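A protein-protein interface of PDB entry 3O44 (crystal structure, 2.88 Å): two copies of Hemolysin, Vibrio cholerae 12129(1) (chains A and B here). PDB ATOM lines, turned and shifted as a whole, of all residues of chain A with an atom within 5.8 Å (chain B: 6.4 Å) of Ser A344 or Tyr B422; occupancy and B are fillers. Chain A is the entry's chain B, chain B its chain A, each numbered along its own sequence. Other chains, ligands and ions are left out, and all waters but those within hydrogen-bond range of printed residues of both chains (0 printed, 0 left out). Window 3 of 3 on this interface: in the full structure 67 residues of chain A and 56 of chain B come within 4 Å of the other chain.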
ATOM      1  N   LEU A 342       4.459   0.935  17.523  1.00  0.00           N
ATOM      2  CA  LEU A 342       3.564   2.020  17.197  1.00  0.00           C
ATOM      3  C   LEU A 342       4.299   2.980  16.275  1.00  0.00           C
ATOM      4  O   LEU A 342       5.165   3.711  16.705  1.00  0.00           O
ATOM      5  CB  LEU A 342       3.096   2.678  18.478  1.00  0.00           C
ATOM      6  CG  LEU A 342       2.637   1.600  19.469  1.00  0.00           C
ATOM      7  CD1 LEU A 342       2.335   2.190  20.843  1.00  0.00           C
ATOM      8  CD2 LEU A 342       1.436   0.781  18.946  1.00  0.00           C
ATOM      9  N   ALA A 343       3.950   2.953  14.997  1.00  0.00           N
ATOM     10  CA  ALA A 343       4.810   3.498  13.951  1.00  0.00           C
ATOM     11  C   ALA A 343       4.617   4.977  13.674  1.00  0.00           C
ATOM     12  O   ALA A 343       5.193   5.511  12.728  1.00  0.00           O
ATOM     13  CB  ALA A 343       4.662   2.693  12.661  1.00  0.00           C
ATOM     14  N   SER A 344       3.795   5.644  14.471  1.00  0.00           N
ATOM     15  CA  SER A 344       3.705   7.088  14.348  1.00  0.00           C
ATOM     16  C   SER A 344       4.933   7.666  15.052  1.00  0.00           C
ATOM     17  O   SER A 344       5.423   8.730  14.690  1.00  0.00           O
ATOM     18  CB  SER A 344       2.421   7.615  14.977  1.00  0.00           C
ATOM     19  OG  SER A 344       2.562   7.732  16.381  1.00  0.00           O
ATOM     20  N   PHE A 345       5.423   6.938  16.056  1.00  0.00           N
ATOM     21  CA  PHE A 345       6.682   7.246  16.729  1.00  0.00           C
ATOM     22  C   PHE A 345       7.875   6.636  16.011  1.00  0.00           C
ATOM     23  O   PHE A 345       7.764   5.594  15.366  1.00  0.00           O
ATOM     24  CB  PHE A 345       6.694   6.668  18.129  1.00  0.00           C
ATOM     25  CG  PHE A 345       5.555   7.103  18.970  1.00  0.00           C
ATOM     26  CD1 PHE A 345       5.647   8.243  19.728  1.00  0.00           C
ATOM     27  CD2 PHE A 345       4.393   6.359  19.022  1.00  0.00           C
ATOM     28  CE1 PHE A 345       4.606   8.645  20.517  1.00  0.00           C
ATOM     29  CE2 PHE A 345       3.343   6.753  19.818  1.00  0.00           C
ATOM     30  CZ  PHE A 345       3.449   7.899  20.562  1.00  0.00           C
ATOM     31  N   ASN A 346       9.036   7.260  16.162  1.00  0.00           N
ATOM     32  CA  ASN A 346      10.233   6.703  15.563  1.00  0.00           C
ATOM     33  C   ASN A 346      10.632   5.439  16.287  1.00  0.00           C
ATOM     34  O   ASN A 346      11.141   4.497  15.678  1.00  0.00           O
ATOM     35  CB  ASN A 346      11.387   7.702  15.585  1.00  0.00           C
ATOM     36  CG  ASN A 346      12.546   7.286  14.677  1.00  0.00           C
ATOM     37  OD1 ASN A 346      12.355   6.684  13.612  1.00  0.00           O
ATOM     38  ND2 ASN A 346      13.762   7.620  15.099  1.00  0.00           N
ATOM     39  N   HIS A 429      -3.267   3.878  17.802  1.00  0.00           N
ATOM     40  CA  HIS A 429      -2.620   4.386  19.011  1.00  0.00           C
ATOM     41  C   HIS A 429      -2.604   5.907  18.990  1.00  0.00           C
ATOM     42  O   HIS A 429      -2.638   6.532  17.917  1.00  0.00           O
ATOM     43  CB  HIS A 429      -1.195   3.829  19.164  1.00  0.00           C
ATOM     44  CG  HIS A 429      -0.279   4.177  18.029  1.00  0.00           C
ATOM     45  ND1 HIS A 429      -0.351   3.555  16.804  1.00  0.00           N
ATOM     46  CD2 HIS A 429       0.715   5.087  17.933  1.00  0.00           C
ATOM     47  CE1 HIS A 429       0.562   4.070  15.997  1.00  0.00           C
ATOM     48  NE2 HIS A 429       1.218   5.002  16.658  1.00  0.00           N
ATOM     49  N   ASP A 430      -2.569   6.494  20.180  1.00  0.00           N
ATOM     50  CA  ASP A 430      -2.559   7.945  20.301  1.00  0.00           C
ATOM     51  C   ASP A 430      -1.179   8.507  19.911  1.00  0.00           C
ATOM     52  O   ASP A 430      -0.157   8.085  20.454  1.00  0.00           O
ATOM     53  CB  ASP A 430      -2.935   8.352  21.734  1.00  0.00           C
ATOM     54  CG  ASP A 430      -3.026   9.853  21.916  1.00  0.00           C
ATOM     55  OD1 ASP A 430      -1.985  10.469  22.225  1.00  0.00           O
ATOM     56  OD2 ASP A 430      -4.132  10.414  21.757  1.00  0.00           O
ATOM     57  N   LYS A 431      -1.153   9.456  18.978  1.00  0.00           N
ATOM     58  CA  LYS A 431       0.107   9.985  18.458  1.00  0.00           C
ATOM     59  C   LYS A 431       1.027  10.550  19.532  1.00  0.00           C
ATOM     60  O   LYS A 431       2.225  10.702  19.292  1.00  0.00           O
ATOM     61  CB  LYS A 431      -0.122  11.034  17.353  1.00  0.00           C
ATOM     62  CG  LYS A 431      -0.679  10.468  16.056  1.00  0.00           C
ATOM     63  CD  LYS A 431      -0.960  11.522  15.007  1.00  0.00           C
ATOM     64  CE  LYS A 431      -1.668  10.897  13.797  1.00  0.00           C
ATOM     65  NZ  LYS A 431      -2.053  11.884  12.750  1.00  0.00           N
ATOM     66  N   GLN A 432       0.479  10.853  20.709  1.00  0.00           N
ATOM     67  CA  GLN A 432       1.270  11.442  21.795  1.00  0.00           C
ATOM     68  C   GLN A 432       1.484  10.506  22.978  1.00  0.00           C
ATOM     69  O   GLN A 432       2.579  10.457  23.536  1.00  0.00           O
ATOM     70  CB  GLN A 432       0.667  12.768  22.276  1.00  0.00           C
ATOM     71  CG  GLN A 432       0.653  13.849  21.205  1.00  0.00           C
ATOM     72  CD  GLN A 432      -0.080  15.099  21.637  1.00  0.00           C
ATOM     73  OE1 GLN A 432      -0.402  15.266  22.815  1.00  0.00           O
ATOM     74  NE2 GLN A 432      -0.348  15.991  20.683  1.00  0.00           N
ATOM     75  N   SER A 447      -3.024   7.183  15.221  1.00  0.00           N
ATOM     76  CA  SER A 447      -2.402   6.540  14.073  1.00  0.00           C
ATOM     77  C   SER A 447      -2.776   5.058  13.993  1.00  0.00           C
ATOM     78  O   SER A 447      -2.854   4.380  15.015  1.00  0.00           O
ATOM     79  CB  SER A 447      -0.892   6.668  14.154  1.00  0.00           C
ATOM     80  OG  SER A 447      -0.290   5.990  13.063  1.00  0.00           O
ATOM     81  N   ARG A 449      -0.988   2.956  12.049  1.00  0.00           N
ATOM     82  CA  ARG A 449       0.214   2.317  11.530  1.00  0.00           C
ATOM     83  C   ARG A 449       0.950   1.493  12.562  1.00  0.00           C
ATOM     84  O   ARG A 449       1.553   2.037  13.460  1.00  0.00           O
ATOM     85  CB  ARG A 449       1.178   3.353  10.970  1.00  0.00           C
ATOM     86  CG  ARG A 449       2.231   2.740  10.113  1.00  0.00           C
ATOM     87  CD  ARG A 449       3.185   3.768   9.587  1.00  0.00           C
ATOM     88  NE  ARG A 449       4.141   3.153   8.676  1.00  0.00           N
ATOM     89  CZ  ARG A 449       5.332   3.661   8.381  1.00  0.00           C
ATOM     90  NH1 ARG A 449       5.725   4.806   8.923  1.00  0.00           N
ATOM     91  NH2 ARG A 449       6.130   3.018   7.541  1.00  0.00           N
ATOM     92  N   ASN B 404      14.990   2.536  15.873  1.00  0.00           N
ATOM     93  CA  ASN B 404      14.469   3.688  15.159  1.00  0.00           C
ATOM     94  C   ASN B 404      13.936   3.304  13.797  1.00  0.00           C
ATOM     95  O   ASN B 404      14.596   2.594  13.044  1.00  0.00           O
ATOM     96  CB  ASN B 404      15.554   4.739  14.961  1.00  0.00           C
ATOM     97  CG  ASN B 404      15.880   5.488  16.224  1.00  0.00           C
ATOM     98  OD1 ASN B 404      15.185   5.372  17.230  1.00  0.00           O
ATOM     99  ND2 ASN B 404      16.939   6.269  16.175  1.00  0.00           N
ATOM    100  N   LEU B 405      12.746   3.787  13.472  1.00  0.00           N
ATOM    101  CA  LEU B 405      12.204   3.546  12.149  1.00  0.00           C
ATOM    102  C   LEU B 405      13.014   4.320  11.129  1.00  0.00           C
ATOM    103  O   LEU B 405      13.040   3.959   9.960  1.00  0.00           O
ATOM    104  CB  LEU B 405      10.723   3.905  12.079  1.00  0.00           C
ATOM    105  CG  LEU B 405       9.848   3.043  12.984  1.00  0.00           C
ATOM    106  CD1 LEU B 405       8.395   3.277  12.720  1.00  0.00           C
ATOM    107  CD2 LEU B 405      10.167   1.601  12.773  1.00  0.00           C
ATOM    108  N   THR B 406      13.697   5.367  11.585  1.00  0.00           N
ATOM    109  CA  THR B 406      14.541   6.163  10.706  1.00  0.00           C
ATOM    110  C   THR B 406      15.816   5.432  10.330  1.00  0.00           C
ATOM    111  O   THR B 406      16.537   5.869   9.434  1.00  0.00           O
ATOM    112  CB  THR B 406      14.915   7.508  11.322  1.00  0.00           C
ATOM    113  OG1 THR B 406      15.481   7.304  12.623  1.00  0.00           O
ATOM    114  CG2 THR B 406      13.697   8.380  11.442  1.00  0.00           C
ATOM    115  N   GLN B 407      16.098   4.326  11.010  1.00  0.00           N
ATOM    116  CA  GLN B 407      17.231   3.483  10.640  1.00  0.00           C
ATOM    117  C   GLN B 407      16.852   2.339   9.685  1.00  0.00           C
ATOM    118  O   GLN B 407      17.690   1.500   9.357  1.00  0.00           O
ATOM    119  CB  GLN B 407      17.912   2.926  11.887  1.00  0.00           C
ATOM    120  CG  GLN B 407      18.801   3.916  12.598  1.00  0.00           C
ATOM    121  CD  GLN B 407      19.480   3.350  13.840  1.00  0.00           C
ATOM    122  OE1 GLN B 407      19.624   2.145  14.006  1.00  0.00           O
ATOM    123  NE2 GLN B 407      19.902   4.233  14.712  1.00  0.00           N
ATOM    124  N   ARG B 408      15.592   2.318   9.240  1.00  0.00           N
ATOM    125  CA  ARG B 408      15.103   1.259   8.341  1.00  0.00           C
ATOM    126  C   ARG B 408      14.814   1.798   6.955  1.00  0.00           C
ATOM    127  O   ARG B 408      14.180   2.832   6.817  1.00  0.00           O
ATOM    128  CB  ARG B 408      13.856   0.562   8.913  1.00  0.00           C
ATOM    129  CG  ARG B 408      14.106  -0.120  10.247  1.00  0.00           C
ATOM    130  CD  ARG B 408      12.878  -0.713  10.838  1.00  0.00           C
ATOM    131  NE  ARG B 408      13.047  -0.940  12.256  1.00  0.00           N
ATOM    132  CZ  ARG B 408      12.163  -1.564  13.022  1.00  0.00           C
ATOM    133  NH1 ARG B 408      11.045  -2.039  12.491  1.00  0.00           N
ATOM    134  NH2 ARG B 408      12.399  -1.725  14.321  1.00  0.00           N
ATOM    135  N   ASN B 420      13.089   5.954   3.275  1.00  0.00           N
ATOM    136  CA  ASN B 420      13.222   5.795   4.710  1.00  0.00           C
ATOM    137  C   ASN B 420      11.882   5.381   5.266  1.00  0.00           C
ATOM    138  O   ASN B 420      10.886   6.024   5.011  1.00  0.00           O
ATOM    139  CB  ASN B 420      13.678   7.107   5.337  1.00  0.00           C
ATOM    140  CG  ASN B 420      14.033   6.969   6.801  1.00  0.00           C
ATOM    141  OD1 ASN B 420      13.237   7.316   7.676  1.00  0.00           O
ATOM    142  ND2 ASN B 420      15.234   6.483   7.076  1.00  0.00           N
ATOM    143  N   VAL B 421      11.868   4.288   6.012  1.00  0.00           N
ATOM    144  CA  VAL B 421      10.636   3.677   6.478  1.00  0.00           C
ATOM    145  C   VAL B 421       9.784   4.636   7.302  1.00  0.00           C
ATOM    146  O   VAL B 421       8.570   4.638   7.214  1.00  0.00           O
ATOM    147  CB  VAL B 421      10.928   2.405   7.294  1.00  0.00           C
ATOM    148  CG1 VAL B 421       9.692   1.952   8.026  1.00  0.00           C
ATOM    149  CG2 VAL B 421      11.430   1.310   6.394  1.00  0.00           C
ATOM    150  N   TYR B 422      10.417   5.464   8.103  1.00  0.00           N
ATOM    151  CA  TYR B 422       9.661   6.328   8.989  1.00  0.00           C
ATOM    152  C   TYR B 422       8.831   7.370   8.253  1.00  0.00           C
ATOM    153  O   TYR B 422       7.621   7.401   8.388  1.00  0.00           O
ATOM    154  CB  TYR B 422      10.601   7.016   9.970  1.00  0.00           C
ATOM    155  CG  TYR B 422       9.890   7.779  11.058  1.00  0.00           C
ATOM    156  CD1 TYR B 422       8.849   7.204  11.771  1.00  0.00           C
ATOM    157  CD2 TYR B 422      10.274   9.065  11.393  1.00  0.00           C
ATOM    158  CE1 TYR B 422       8.208   7.890  12.772  1.00  0.00           C
ATOM    159  CE2 TYR B 422       9.633   9.762  12.393  1.00  0.00           C
ATOM    160  CZ  TYR B 422       8.600   9.172  13.079  1.00  0.00           C
ATOM    161  OH  TYR B 422       7.969   9.877  14.074  1.00  0.00           O
ATOM    162  N   SER B 423       9.486   8.224   7.478  1.00  0.00           N
ATOM    163  CA  SER B 423       8.821   9.345   6.820  1.00  0.00           C
ATOM    164  C   SER B 423       8.353   9.023   5.415  1.00  0.00           C
ATOM    165  O   SER B 423       7.487   9.709   4.878  1.00  0.00           O
ATOM    166  CB  SER B 423       9.760  10.553   6.758  1.00  0.00           C
ATOM    167  OG  SER B 423      10.994  10.209   6.152  1.00  0.00           O
ATOM    168  N   GLY B 424       8.934   7.993   4.809  1.00  0.00           N
ATOM    169  CA  GLY B 424       8.602   7.643   3.442  1.00  0.00           C
ATOM    170  C   GLY B 424       9.408   8.426   2.429  1.00  0.00           C
ATOM    171  O   GLY B 424       9.397   8.138   1.236  1.00  0.00           O
ATOM    172  N   GLU B 425      10.123   9.430   2.909  1.00  0.00           N
ATOM    173  CA  GLU B 425      10.983  10.239   2.048  1.00  0.00           C
ATOM    174  C   GLU B 425      12.140   9.409   1.471  1.00  0.00           C
ATOM    175  O   GLU B 425      12.452   8.325   1.964  1.00  0.00           O
ATOM    176  CB  GLU B 425      11.505  11.447   2.820  1.00  0.00           C
ATOM    177  CG  GLU B 425      10.405  12.369   3.348  1.00  0.00           C
ATOM    178  CD  GLU B 425      10.941  13.640   4.028  1.00  0.00           C
ATOM    179  OE1 GLU B 425      11.557  13.538   5.115  1.00  0.00           O
ATOM    180  OE2 GLU B 425      10.733  14.745   3.478  1.00  0.00           O
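Leu B405 touches Ala A343.
Ala A343 touches Tyr B422 (O to CE1, 3.8 Å).
O of Phe A345 touches CD1 of Leu B405, at 3.6 Å.
Tyr B422 touches Phe A345 (CE1 to C, 3.5 Å).
Asn A346 touches Tyr B422.
The side-chain amide nitrogen (ND2) of Asn B420 sits at hydrogen-bond distance from the backbone carbonyl oxygen (O) of Thr B406.
The backbone carbonyl oxygen (O) of Arg B408 lies within hydrogen-bond range of the backbone NH (N) of Val B421 (2.8 Å).
N of Tyr B422 lies close to OD1 of Asn B420 (3.4 Å).
N of Ala A343 lies within hydrogen-bond range of O of Arg A449, at 3.0 Å.
The side-chain hydroxyl (OG) of Ser A344 lies within hydrogen-bond range of a ring nitrogen (NE2) of His A429, at 3.1 Å.
OG of Ser A447 is in hydrogen-bond range of N of Arg A449, 3.3 Å away.
No position is printed for both chains.
Of the 11 pairs that touch across the chains among the printed residues, none has its exchanged pair printed and touching as well.
The side-chain amide oxygen of Asn B404 lies close to the side-chain amide nitrogen of Asn A346 (3.4 Å).
The backbone NH of Leu B405 sits at hydrogen-bond distance from the backbone carbonyl oxygen of Asn A346 (2.8 Å).
N of Thr B406 sits at hydrogen-bond distance from OD1 of Asn A346 (2.8 Å).
The backbone carbonyl oxygen (O) of Val B421 lies within hydrogen-bond range of the guanidinium group (NH2) of Arg A449, 2.9 Å away.
The side-chain hydroxyl (OH) of Tyr B422 sits at hydrogen-bond distance from the backbone carbonyl oxygen (O) of Ser A344 (2.9 Å).
The backbone carbonyl oxygen (O) of Tyr B422 lies within hydrogen-bond range of the guanidinium group (NH1) of Arg A449, at 3.3 Å.
Along chain A the printed residues that touch a printed residue of chain B span positions 343 to 449.
Among the printed residues, 11 pairs touch across the chains.
Of chain B, only Tyr B422 comes within 4 Å of Ser A344.
Of chain A, only Ala A343, Ser A344, Phe A345, Asn A346 and Arg A449 come within 4 Å of Tyr B422.
Of the printed residues of chain A, Asn B404 touches Asn A346 (3.2 Å).
Printed residues of chain A within 4 Å of Leu B405: Ala A343, Phe A345 and Asn A346.
Glu B425 touches none of the printed residues of chain A.
The nearest residue of chain B that does not touch Ser A344 is Leu B405 (5.5 Å).
The nearest printed residue of chain B that does not touch Ala A343 is Val B421 (6.5 Å).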
